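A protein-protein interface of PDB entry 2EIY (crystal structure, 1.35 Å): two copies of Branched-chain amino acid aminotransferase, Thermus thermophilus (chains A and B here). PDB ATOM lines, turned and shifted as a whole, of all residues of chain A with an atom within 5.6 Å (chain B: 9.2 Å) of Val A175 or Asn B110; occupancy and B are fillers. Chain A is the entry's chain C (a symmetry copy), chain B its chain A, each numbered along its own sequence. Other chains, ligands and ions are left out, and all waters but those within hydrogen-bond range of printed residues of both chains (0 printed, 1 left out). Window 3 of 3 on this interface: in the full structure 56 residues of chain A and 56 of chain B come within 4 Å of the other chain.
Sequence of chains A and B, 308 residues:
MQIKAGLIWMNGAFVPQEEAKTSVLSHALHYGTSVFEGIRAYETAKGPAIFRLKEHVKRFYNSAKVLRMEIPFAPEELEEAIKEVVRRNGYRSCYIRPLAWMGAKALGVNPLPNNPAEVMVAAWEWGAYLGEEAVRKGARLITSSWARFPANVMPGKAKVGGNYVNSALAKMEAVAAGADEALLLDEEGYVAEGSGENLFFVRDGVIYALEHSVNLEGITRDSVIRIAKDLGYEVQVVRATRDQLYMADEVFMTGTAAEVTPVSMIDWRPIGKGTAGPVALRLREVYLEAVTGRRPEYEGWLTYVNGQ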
ATOM      1  N   ALA A 168      14.706   7.128 -11.993  1.00  0.00           N
ATOM      2  CA  ALA A 168      14.911   8.391 -12.695  1.00  0.00           C
ATOM      3  C   ALA A 168      13.622   8.906 -13.327  1.00  0.00           C
ATOM      4  O   ALA A 168      13.310  10.093 -13.238  1.00  0.00           O
ATOM      5  CB  ALA A 168      15.981   8.226 -13.767  1.00  0.00           C
ATOM      6  N   ALA A 170      10.534   8.213 -12.463  1.00  0.00           N
ATOM      7  CA  ALA A 170       9.608   8.611 -11.415  1.00  0.00           C
ATOM      8  C   ALA A 170      10.025   9.935 -10.778  1.00  0.00           C
ATOM      9  O   ALA A 170       9.187  10.806 -10.547  1.00  0.00           O
ATOM     10  CB  ALA A 170       9.518   7.518 -10.356  1.00  0.00           C
ATOM     11  N   LYS A 171      11.319  10.097 -10.506  1.00  0.00           N
ATOM     12  CA  LYS A 171      11.805  11.328  -9.890  1.00  0.00           C
ATOM     13  C   LYS A 171      11.567  12.536 -10.792  1.00  0.00           C
ATOM     14  O   LYS A 171      11.115  13.582 -10.327  1.00  0.00           O
ATOM     15  CB  LYS A 171      13.298  11.204  -9.557  1.00  0.00           C
ATOM     16  CG  LYS A 171      13.878  12.398  -8.805  1.00  0.00           C
ATOM     17  CD  LYS A 171      13.126  12.657  -7.506  1.00  0.00           C
ATOM     18  CE  LYS A 171      13.772  13.779  -6.698  1.00  0.00           C
ATOM     19  NZ  LYS A 171      15.137  13.417  -6.227  1.00  0.00           N
ATOM     20  N   MET A 172      11.868  12.402 -12.081  1.00  0.00           N
ATOM     21  CA  MET A 172      11.658  13.513 -13.007  1.00  0.00           C
ATOM     22  C   MET A 172      10.190  13.908 -13.039  1.00  0.00           C
ATOM     23  O   MET A 172       9.857  15.092 -13.058  1.00  0.00           O
ATOM     24  CB  MET A 172      12.099  13.147 -14.426  1.00  0.00           C
ATOM     25  CG  MET A 172      13.599  13.092 -14.638  1.00  0.00           C
ATOM     26  SD  MET A 172      14.009  12.986 -16.396  1.00  0.00           S
ATOM     27  CE  MET A 172      13.567  11.270 -16.729  1.00  0.00           C
ATOM     28  N   GLU A 173       9.315  12.908 -13.055  1.00  0.00           N
ATOM     29  CA  GLU A 173       7.877  13.138 -13.080  1.00  0.00           C
ATOM     30  C   GLU A 173       7.423  13.916 -11.845  1.00  0.00           C
ATOM     31  O   GLU A 173       6.657  14.879 -11.946  1.00  0.00           O
ATOM     32  CB  GLU A 173       7.140  11.795 -13.147  1.00  0.00           C
ATOM     33  CG  GLU A 173       5.624  11.924 -13.114  1.00  0.00           C
ATOM     34  CD  GLU A 173       4.905  10.585 -13.098  1.00  0.00           C
ATOM     35  OE1 GLU A 173       3.797  10.506 -13.666  1.00  0.00           O
ATOM     36  OE2 GLU A 173       5.435   9.621 -12.514  1.00  0.00           O
ATOM     37  N   ALA A 174       7.906  13.499 -10.679  1.00  0.00           N
ATOM     38  CA  ALA A 174       7.540  14.150  -9.428  1.00  0.00           C
ATOM     39  C   ALA A 174       7.990  15.606  -9.406  1.00  0.00           C
ATOM     40  O   ALA A 174       7.220  16.500  -9.053  1.00  0.00           O
ATOM     41  CB  ALA A 174       8.151  13.397  -8.256  1.00  0.00           C
ATOM     42  N   VAL A 175       9.237  15.842  -9.791  1.00  0.00           N
ATOM     43  CA  VAL A 175       9.773  17.195  -9.805  1.00  0.00           C
ATOM     44  C   VAL A 175       9.035  18.075 -10.814  1.00  0.00           C
ATOM     45  O   VAL A 175       8.741  19.240 -10.534  1.00  0.00           O
ATOM     46  CB  VAL A 175      11.285  17.186 -10.116  1.00  0.00           C
ATOM     47  CG1 VAL A 175      11.801  18.612 -10.268  1.00  0.00           C
ATOM     48  CG2 VAL A 175      12.034  16.480  -8.996  1.00  0.00           C
ATOM     49  N   ALA A 176       8.725  17.522 -11.982  1.00  0.00           N
ATOM     50  CA  ALA A 176       8.016  18.279 -13.009  1.00  0.00           C
ATOM     51  C   ALA A 176       6.611  18.654 -12.544  1.00  0.00           C
ATOM     52  O   ALA A 176       6.065  19.685 -12.946  1.00  0.00           O
ATOM     53  CB  ALA A 176       7.935  17.465 -14.293  1.00  0.00           C
ATOM     54  N   ALA A 177       6.026  17.812 -11.698  1.00  0.00           N
ATOM     55  CA  ALA A 177       4.683  18.048 -11.181  1.00  0.00           C
ATOM     56  C   ALA A 177       4.684  19.034 -10.016  1.00  0.00           C
ATOM     57  O   ALA A 177       3.624  19.405  -9.509  1.00  0.00           O
ATOM     58  CB  ALA A 177       4.055  16.724 -10.746  1.00  0.00           C
ATOM     59  N   GLY A 178       5.874  19.450  -9.590  1.00  0.00           N
ATOM     60  CA  GLY A 178       5.980  20.400  -8.497  1.00  0.00           C
ATOM     61  C   GLY A 178       6.243  19.807  -7.125  1.00  0.00           C
ATOM     62  O   GLY A 178       6.199  20.520  -6.123  1.00  0.00           O
ATOM     63  N   ALA A 179       6.524  18.508  -7.068  1.00  0.00           N
ATOM     64  CA  ALA A 179       6.791  17.841  -5.797  1.00  0.00           C
ATOM     65  C   ALA A 179       8.291  17.678  -5.555  1.00  0.00           C
ATOM     66  O   ALA A 179       9.108  18.018  -6.412  1.00  0.00           O
ATOM     67  CB  ALA A 179       6.106  16.476  -5.773  1.00  0.00           C
ATOM     68  N   ASP A 180       8.646  17.164  -4.381  1.00  0.00           N
ATOM     69  CA  ASP A 180      10.046  16.954  -4.024  1.00  0.00           C
ATOM     70  C   ASP A 180      10.512  15.545  -4.335  1.00  0.00           C
ATOM     71  O   ASP A 180      11.687  15.319  -4.625  1.00  0.00           O
ATOM     72  CB  ASP A 180      10.268  17.190  -2.530  1.00  0.00           C
ATOM     73  CG  ASP A 180       9.897  18.588  -2.096  1.00  0.00           C
ATOM     74  OD1 ASP A 180      10.475  19.554  -2.639  1.00  0.00           O
ATOM     75  OD2 ASP A 180       9.034  18.717  -1.205  1.00  0.00           O
ATOM     76  N   HIS B  27      26.605   9.611 -14.873  1.00  0.00           N
ATOM     77  CA  HIS B  27      25.269   9.213 -14.433  1.00  0.00           C
ATOM     78  C   HIS B  27      24.852   7.868 -15.035  1.00  0.00           C
ATOM     79  O   HIS B  27      24.341   6.996 -14.331  1.00  0.00           O
ATOM     80  CB  HIS B  27      24.273  10.310 -14.833  1.00  0.00           C
ATOM     81  CG  HIS B  27      22.969  10.268 -14.093  1.00  0.00           C
ATOM     82  ND1 HIS B  27      21.906   9.486 -14.492  1.00  0.00           N
ATOM     83  CD2 HIS B  27      22.544  10.954 -13.005  1.00  0.00           C
ATOM     84  CE1 HIS B  27      20.881   9.695 -13.684  1.00  0.00           C
ATOM     85  NE2 HIS B  27      21.243  10.582 -12.773  1.00  0.00           N
ATOM     86  N   TYR B  31      23.304   4.670 -13.131  1.00  0.00           N
ATOM     87  CA  TYR B  31      21.852   4.548 -13.192  1.00  0.00           C
ATOM     88  C   TYR B  31      21.208   4.080 -14.503  1.00  0.00           C
ATOM     89  O   TYR B  31      19.986   4.187 -14.664  1.00  0.00           O
ATOM     90  CB  TYR B  31      21.240   5.891 -12.768  1.00  0.00           C
ATOM     91  CG  TYR B  31      21.806   6.460 -11.476  1.00  0.00           C
ATOM     92  CD1 TYR B  31      22.340   7.752 -11.436  1.00  0.00           C
ATOM     93  CD2 TYR B  31      21.789   5.721 -10.290  1.00  0.00           C
ATOM     94  CE1 TYR B  31      22.840   8.292 -10.248  1.00  0.00           C
ATOM     95  CE2 TYR B  31      22.287   6.255  -9.097  1.00  0.00           C
ATOM     96  CZ  TYR B  31      22.810   7.541  -9.085  1.00  0.00           C
ATOM     97  OH  TYR B  31      23.299   8.073  -7.909  1.00  0.00           O
ATOM     98  N   THR B  33      21.160   5.338 -17.419  1.00  0.00           N
ATOM     99  CA  THR B  33      20.609   6.420 -18.217  1.00  0.00           C
ATOM    100  C   THR B  33      21.338   6.715 -19.528  1.00  0.00           C
ATOM    101  O   THR B  33      21.923   7.784 -19.714  1.00  0.00           O
ATOM    102  CB  THR B  33      20.536   7.694 -17.365  1.00  0.00           C
ATOM    103  OG1 THR B  33      21.767   7.844 -16.646  1.00  0.00           O
ATOM    104  CG2 THR B  33      19.380   7.599 -16.361  1.00  0.00           C
ATOM    105  N   LEU B  67      13.678   9.527 -22.050  1.00  0.00           N
ATOM    106  CA  LEU B  67      14.431   9.885 -20.850  1.00  0.00           C
ATOM    107  C   LEU B  67      14.554  11.396 -20.692  1.00  0.00           C
ATOM    108  O   LEU B  67      15.226  11.868 -19.777  1.00  0.00           O
ATOM    109  CB  LEU B  67      15.842   9.298 -20.910  1.00  0.00           C
ATOM    110  CG  LEU B  67      16.012   7.783 -20.864  1.00  0.00           C
ATOM    111  CD1 LEU B  67      17.489   7.443 -21.013  1.00  0.00           C
ATOM    112  CD2 LEU B  67      15.465   7.246 -19.550  1.00  0.00           C
ATOM    113  N   ARG B  68      13.902  12.143 -21.579  1.00  0.00           N
ATOM    114  CA  ARG B  68      13.979  13.602 -21.566  1.00  0.00           C
ATOM    115  C   ARG B  68      15.447  14.002 -21.680  1.00  0.00           C
ATOM    116  O   ARG B  68      15.899  15.004 -21.118  1.00  0.00           O
ATOM    117  CB  ARG B  68      13.341  14.175 -20.297  1.00  0.00           C
ATOM    118  CG  ARG B  68      11.830  13.963 -20.259  1.00  0.00           C
ATOM    119  CD  ARG B  68      11.177  14.649 -19.067  1.00  0.00           C
ATOM    120  NE  ARG B  68      11.321  16.100 -19.123  1.00  0.00           N
ATOM    121  CZ  ARG B  68      10.961  16.922 -18.144  1.00  0.00           C
ATOM    122  NH1 ARG B  68      10.432  16.436 -17.028  1.00  0.00           N
ATOM    123  NH2 ARG B  68      11.143  18.229 -18.275  1.00  0.00           N
ATOM    124  N   MET B 102      24.132  10.033 -20.133  1.00  0.00           N
ATOM    125  CA  MET B 102      24.167  11.152 -19.203  1.00  0.00           C
ATOM    126  C   MET B 102      25.535  11.164 -18.535  1.00  0.00           C
ATOM    127  O   MET B 102      26.000  10.141 -18.021  1.00  0.00           O
ATOM    128  CB  MET B 102      23.055  11.017 -18.159  1.00  0.00           C
ATOM    129  CG  MET B 102      21.651  11.064 -18.751  1.00  0.00           C
ATOM    130  SD  MET B 102      21.408  12.426 -19.928  1.00  0.00           S
ATOM    131  CE  MET B 102      21.395  13.812 -18.855  1.00  0.00           C
ATOM    132  N   GLY B 103      26.170  12.334 -18.556  1.00  0.00           N
ATOM    133  CA  GLY B 103      27.504  12.506 -18.004  1.00  0.00           C
ATOM    134  C   GLY B 103      27.676  12.637 -16.502  1.00  0.00           C
ATOM    135  O   GLY B 103      26.773  12.331 -15.726  1.00  0.00           O
ATOM    136  N   LYS B 105      28.012  15.408 -14.471  1.00  0.00           N
ATOM    137  CA  LYS B 105      27.766  16.709 -13.854  1.00  0.00           C
ATOM    138  C   LYS B 105      27.278  16.549 -12.415  1.00  0.00           C
ATOM    139  O   LYS B 105      27.610  17.353 -11.545  1.00  0.00           O
ATOM    140  CB  LYS B 105      26.737  17.503 -14.660  1.00  0.00           C
ATOM    141  CG  LYS B 105      27.292  18.124 -15.932  1.00  0.00           C
ATOM    142  CD  LYS B 105      26.230  18.922 -16.664  1.00  0.00           C
ATOM    143  CE  LYS B 105      26.807  19.605 -17.893  1.00  0.00           C
ATOM    144  NZ  LYS B 105      25.780  20.403 -18.615  1.00  0.00           N
ATOM    145  N   ALA B 106      26.492  15.505 -12.170  1.00  0.00           N
ATOM    146  CA  ALA B 106      25.955  15.236 -10.841  1.00  0.00           C
ATOM    147  C   ALA B 106      25.486  13.789 -10.768  1.00  0.00           C
ATOM    148  O   ALA B 106      25.331  13.132 -11.799  1.00  0.00           O
ATOM    149  CB  ALA B 106      24.794  16.177 -10.550  1.00  0.00           C
ATOM    150  N   LEU B 107      25.259  13.294  -9.555  1.00  0.00           N
ATOM    151  CA  LEU B 107      24.806  11.919  -9.391  1.00  0.00           C
ATOM    152  C   LEU B 107      23.490  11.757  -8.639  1.00  0.00           C
ATOM    153  O   LEU B 107      23.262  10.746  -7.970  1.00  0.00           O
ATOM    154  CB  LEU B 107      25.908  11.067  -8.752  1.00  0.00           C
ATOM    155  CG  LEU B 107      27.008  10.636  -9.736  1.00  0.00           C
ATOM    156  CD1 LEU B 107      28.121   9.908  -8.996  1.00  0.00           C
ATOM    157  CD2 LEU B 107      26.404   9.731 -10.809  1.00  0.00           C
ATOM    158  N   GLY B 108      22.627  12.763  -8.740  1.00  0.00           N
ATOM    159  CA  GLY B 108      21.314  12.650  -8.133  1.00  0.00           C
ATOM    160  C   GLY B 108      20.595  11.728  -9.106  1.00  0.00           C
ATOM    161  O   GLY B 108      20.962  11.687 -10.282  1.00  0.00           O
ATOM    162  N   VAL B 109      19.588  10.988  -8.659  1.00  0.00           N
ATOM    163  CA  VAL B 109      18.904  10.073  -9.571  1.00  0.00           C
ATOM    164  C   VAL B 109      18.271  10.789 -10.768  1.00  0.00           C
ATOM    165  O   VAL B 109      18.230  10.241 -11.871  1.00  0.00           O
ATOM    166  CB  VAL B 109      17.832   9.231  -8.833  1.00  0.00           C
ATOM    167  CG1 VAL B 109      16.671  10.104  -8.401  1.00  0.00           C
ATOM    168  CG2 VAL B 109      17.360   8.104  -9.732  1.00  0.00           C
ATOM    169  N   ASN B 110      17.783  12.009 -10.554  1.00  0.00           N
ATOM    170  CA  ASN B 110      17.180  12.798 -11.630  1.00  0.00           C
ATOM    171  C   ASN B 110      18.303  13.143 -12.613  1.00  0.00           C
ATOM    172  O   ASN B 110      19.284  13.782 -12.240  1.00  0.00           O
ATOM    173  CB  ASN B 110      16.581  14.090 -11.062  1.00  0.00           C
ATOM    174  CG  ASN B 110      15.798  14.879 -12.096  1.00  0.00           C
ATOM    175  OD1 ASN B 110      16.044  14.772 -13.297  1.00  0.00           O
ATOM    176  ND2 ASN B 110      14.856  15.693 -11.628  1.00  0.00           N
ATOM    177  N   PRO B 111      18.172  12.729 -13.881  1.00  0.00           N
ATOM    178  CA  PRO B 111      19.211  13.015 -14.877  1.00  0.00           C
ATOM    179  C   PRO B 111      19.145  14.378 -15.572  1.00  0.00           C
ATOM    180  O   PRO B 111      20.088  14.761 -16.262  1.00  0.00           O
ATOM    181  CB  PRO B 111      19.047  11.868 -15.867  1.00  0.00           C
ATOM    182  CG  PRO B 111      17.566  11.698 -15.895  1.00  0.00           C
ATOM    183  CD  PRO B 111      17.172  11.788 -14.424  1.00  0.00           C
ATOM    184  N   LEU B 112      18.049  15.108 -15.400  1.00  0.00           N
ATOM    185  CA  LEU B 112      17.908  16.406 -16.058  1.00  0.00           C
ATOM    186  C   LEU B 112      19.076  17.376 -15.858  1.00  0.00           C
ATOM    187  O   LEU B 112      19.514  18.025 -16.808  1.00  0.00           O
ATOM    188  CB  LEU B 112      16.593  17.066 -15.638  1.00  0.00           C
ATOM    189  CG  LEU B 112      15.346  16.321 -16.124  1.00  0.00           C
ATOM    190  CD1 LEU B 112      14.098  17.016 -15.605  1.00  0.00           C
ATOM    191  CD2 LEU B 112      15.342  16.260 -17.646  1.00  0.00           C
ATOM    192  N   PRO B 113      19.596  17.493 -14.625  1.00  0.00           N
ATOM    193  CA  PRO B 113      20.717  18.411 -14.393  1.00  0.00           C
ATOM    194  C   PRO B 113      21.968  18.040 -15.193  1.00  0.00           C
ATOM    195  O   PRO B 113      22.884  18.853 -15.342  1.00  0.00           O
ATOM    196  CB  PRO B 113      20.956  18.291 -12.889  1.00  0.00           C
ATOM    197  CG  PRO B 113      19.595  17.980 -12.357  1.00  0.00           C
ATOM    198  CD  PRO B 113      19.084  16.963 -13.347  1.00  0.00           C
ATOM    199  N   ASN B 114      21.998  16.814 -15.708  1.00  0.00           N
ATOM    200  CA  ASN B 114      23.146  16.327 -16.467  1.00  0.00           C
ATOM    201  C   ASN B 114      23.108  16.615 -17.965  1.00  0.00           C
ATOM    202  O   ASN B 114      24.092  16.367 -18.662  1.00  0.00           O
ATOM    203  CB  ASN B 114      23.313  14.820 -16.244  1.00  0.00           C
ATOM    204  CG  ASN B 114      23.554  14.467 -14.787  1.00  0.00           C
ATOM    205  OD1 ASN B 114      22.707  14.710 -13.925  1.00  0.00           O
ATOM    206  ND2 ASN B 114      24.713  13.891 -14.504  1.00  0.00           N
ATOM    207  N   ASN B 115      21.985  17.126 -18.464  1.00  0.00           N
ATOM    208  CA  ASN B 115      21.869  17.437 -19.888  1.00  0.00           C
ATOM    209  C   ASN B 115      22.833  18.555 -20.268  1.00  0.00           C
ATOM    210  O   ASN B 115      23.169  19.398 -19.441  1.00  0.00           O
ATOM    211  CB  ASN B 115      20.439  17.858 -20.242  1.00  0.00           C
ATOM    212  CG  ASN B 115      19.553  16.677 -20.591  1.00  0.00           C
ATOM    213  OD1 ASN B 115      19.939  15.814 -21.375  1.00  0.00           O
ATOM    214  ND2 ASN B 115      18.355  16.642 -20.022  1.00  0.00           N
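The backbone carbonyl oxygen (O) of Leu B67 sits close to the side-chain sulfur (SD) of Met A172 (3.8 Å).
Val A175 touches just one residue of chain B: Asn B110.
Ala A176 touches just one residue of chain B: Arg B68 (3.8 Å).
Of the printed residues of chain A, Pro B111 touches Ala A168 and Met A172.
Printed residues of chain B within 4 Å of Met A172: Leu B67, Asn B110, Pro B111 and Leu B112.
Lys B105 touches none of the printed residues of chain A.
Tyr B31 touches none of the printed residues of chain A.
The nearest residue of chain B that does not touch Val A175 is Leu B112 (6.0 Å).
The nearest residue of chain A that does not touch Asn B110 is Ala A168 (5.0 Å).
No position is printed for both chains.
Of the 10 pairs that touch across the chains among the printed residues, none has its exchanged pair printed and touching as well.
A ring nitrogen (NE2) of His B27 lies within hydrogen-bond range of the backbone carbonyl oxygen of Val B109 (3.2 Å).
O of Arg B68 lies within hydrogen-bond range of ND2 of Asn B115, at 3.1 Å.
The backbone NH of Leu B112 sits at hydrogen-bond distance from the side-chain amide oxygen of Asn B110, 2.9 Å away.
Ala A168 touches Val B109.
CD of Pro B111 touches CB of Ala A168, at 3.8 Å.
Lys A171 touches Val B109.
CG of Lys A171 touches CB of Asn B110 (3.9 Å).
Asn B110 touches Met A172.
Met A172 touches Pro B111 (CG to CD, 3.8 Å).
CG of Leu B112 touches SD of Met A172, at 3.6 Å.
ND2 of Asn B110 touches CG2 of Val A175 (3.9 Å).
CB of Ala A176 touches NH1 of Arg B68 (3.8 Å).
Of the 12 printed residues of chain A, 5 touch a printed residue of chain B.
Printed residues of chain A that touch a printed residue of chain B: Ala A168, Lys A171, Met A172, Val A175 and Ala A176.
Of the 18 printed residues of chain B, 6 touch a printed residue of chain A.
Along chain B the printed residues that touch a printed residue of chain A span positions 67 to 112.
Among the printed residues, no Asp or Glu carboxylate lies within 4 Å of a Lys or Arg side-chain nitrogen of the other chain.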
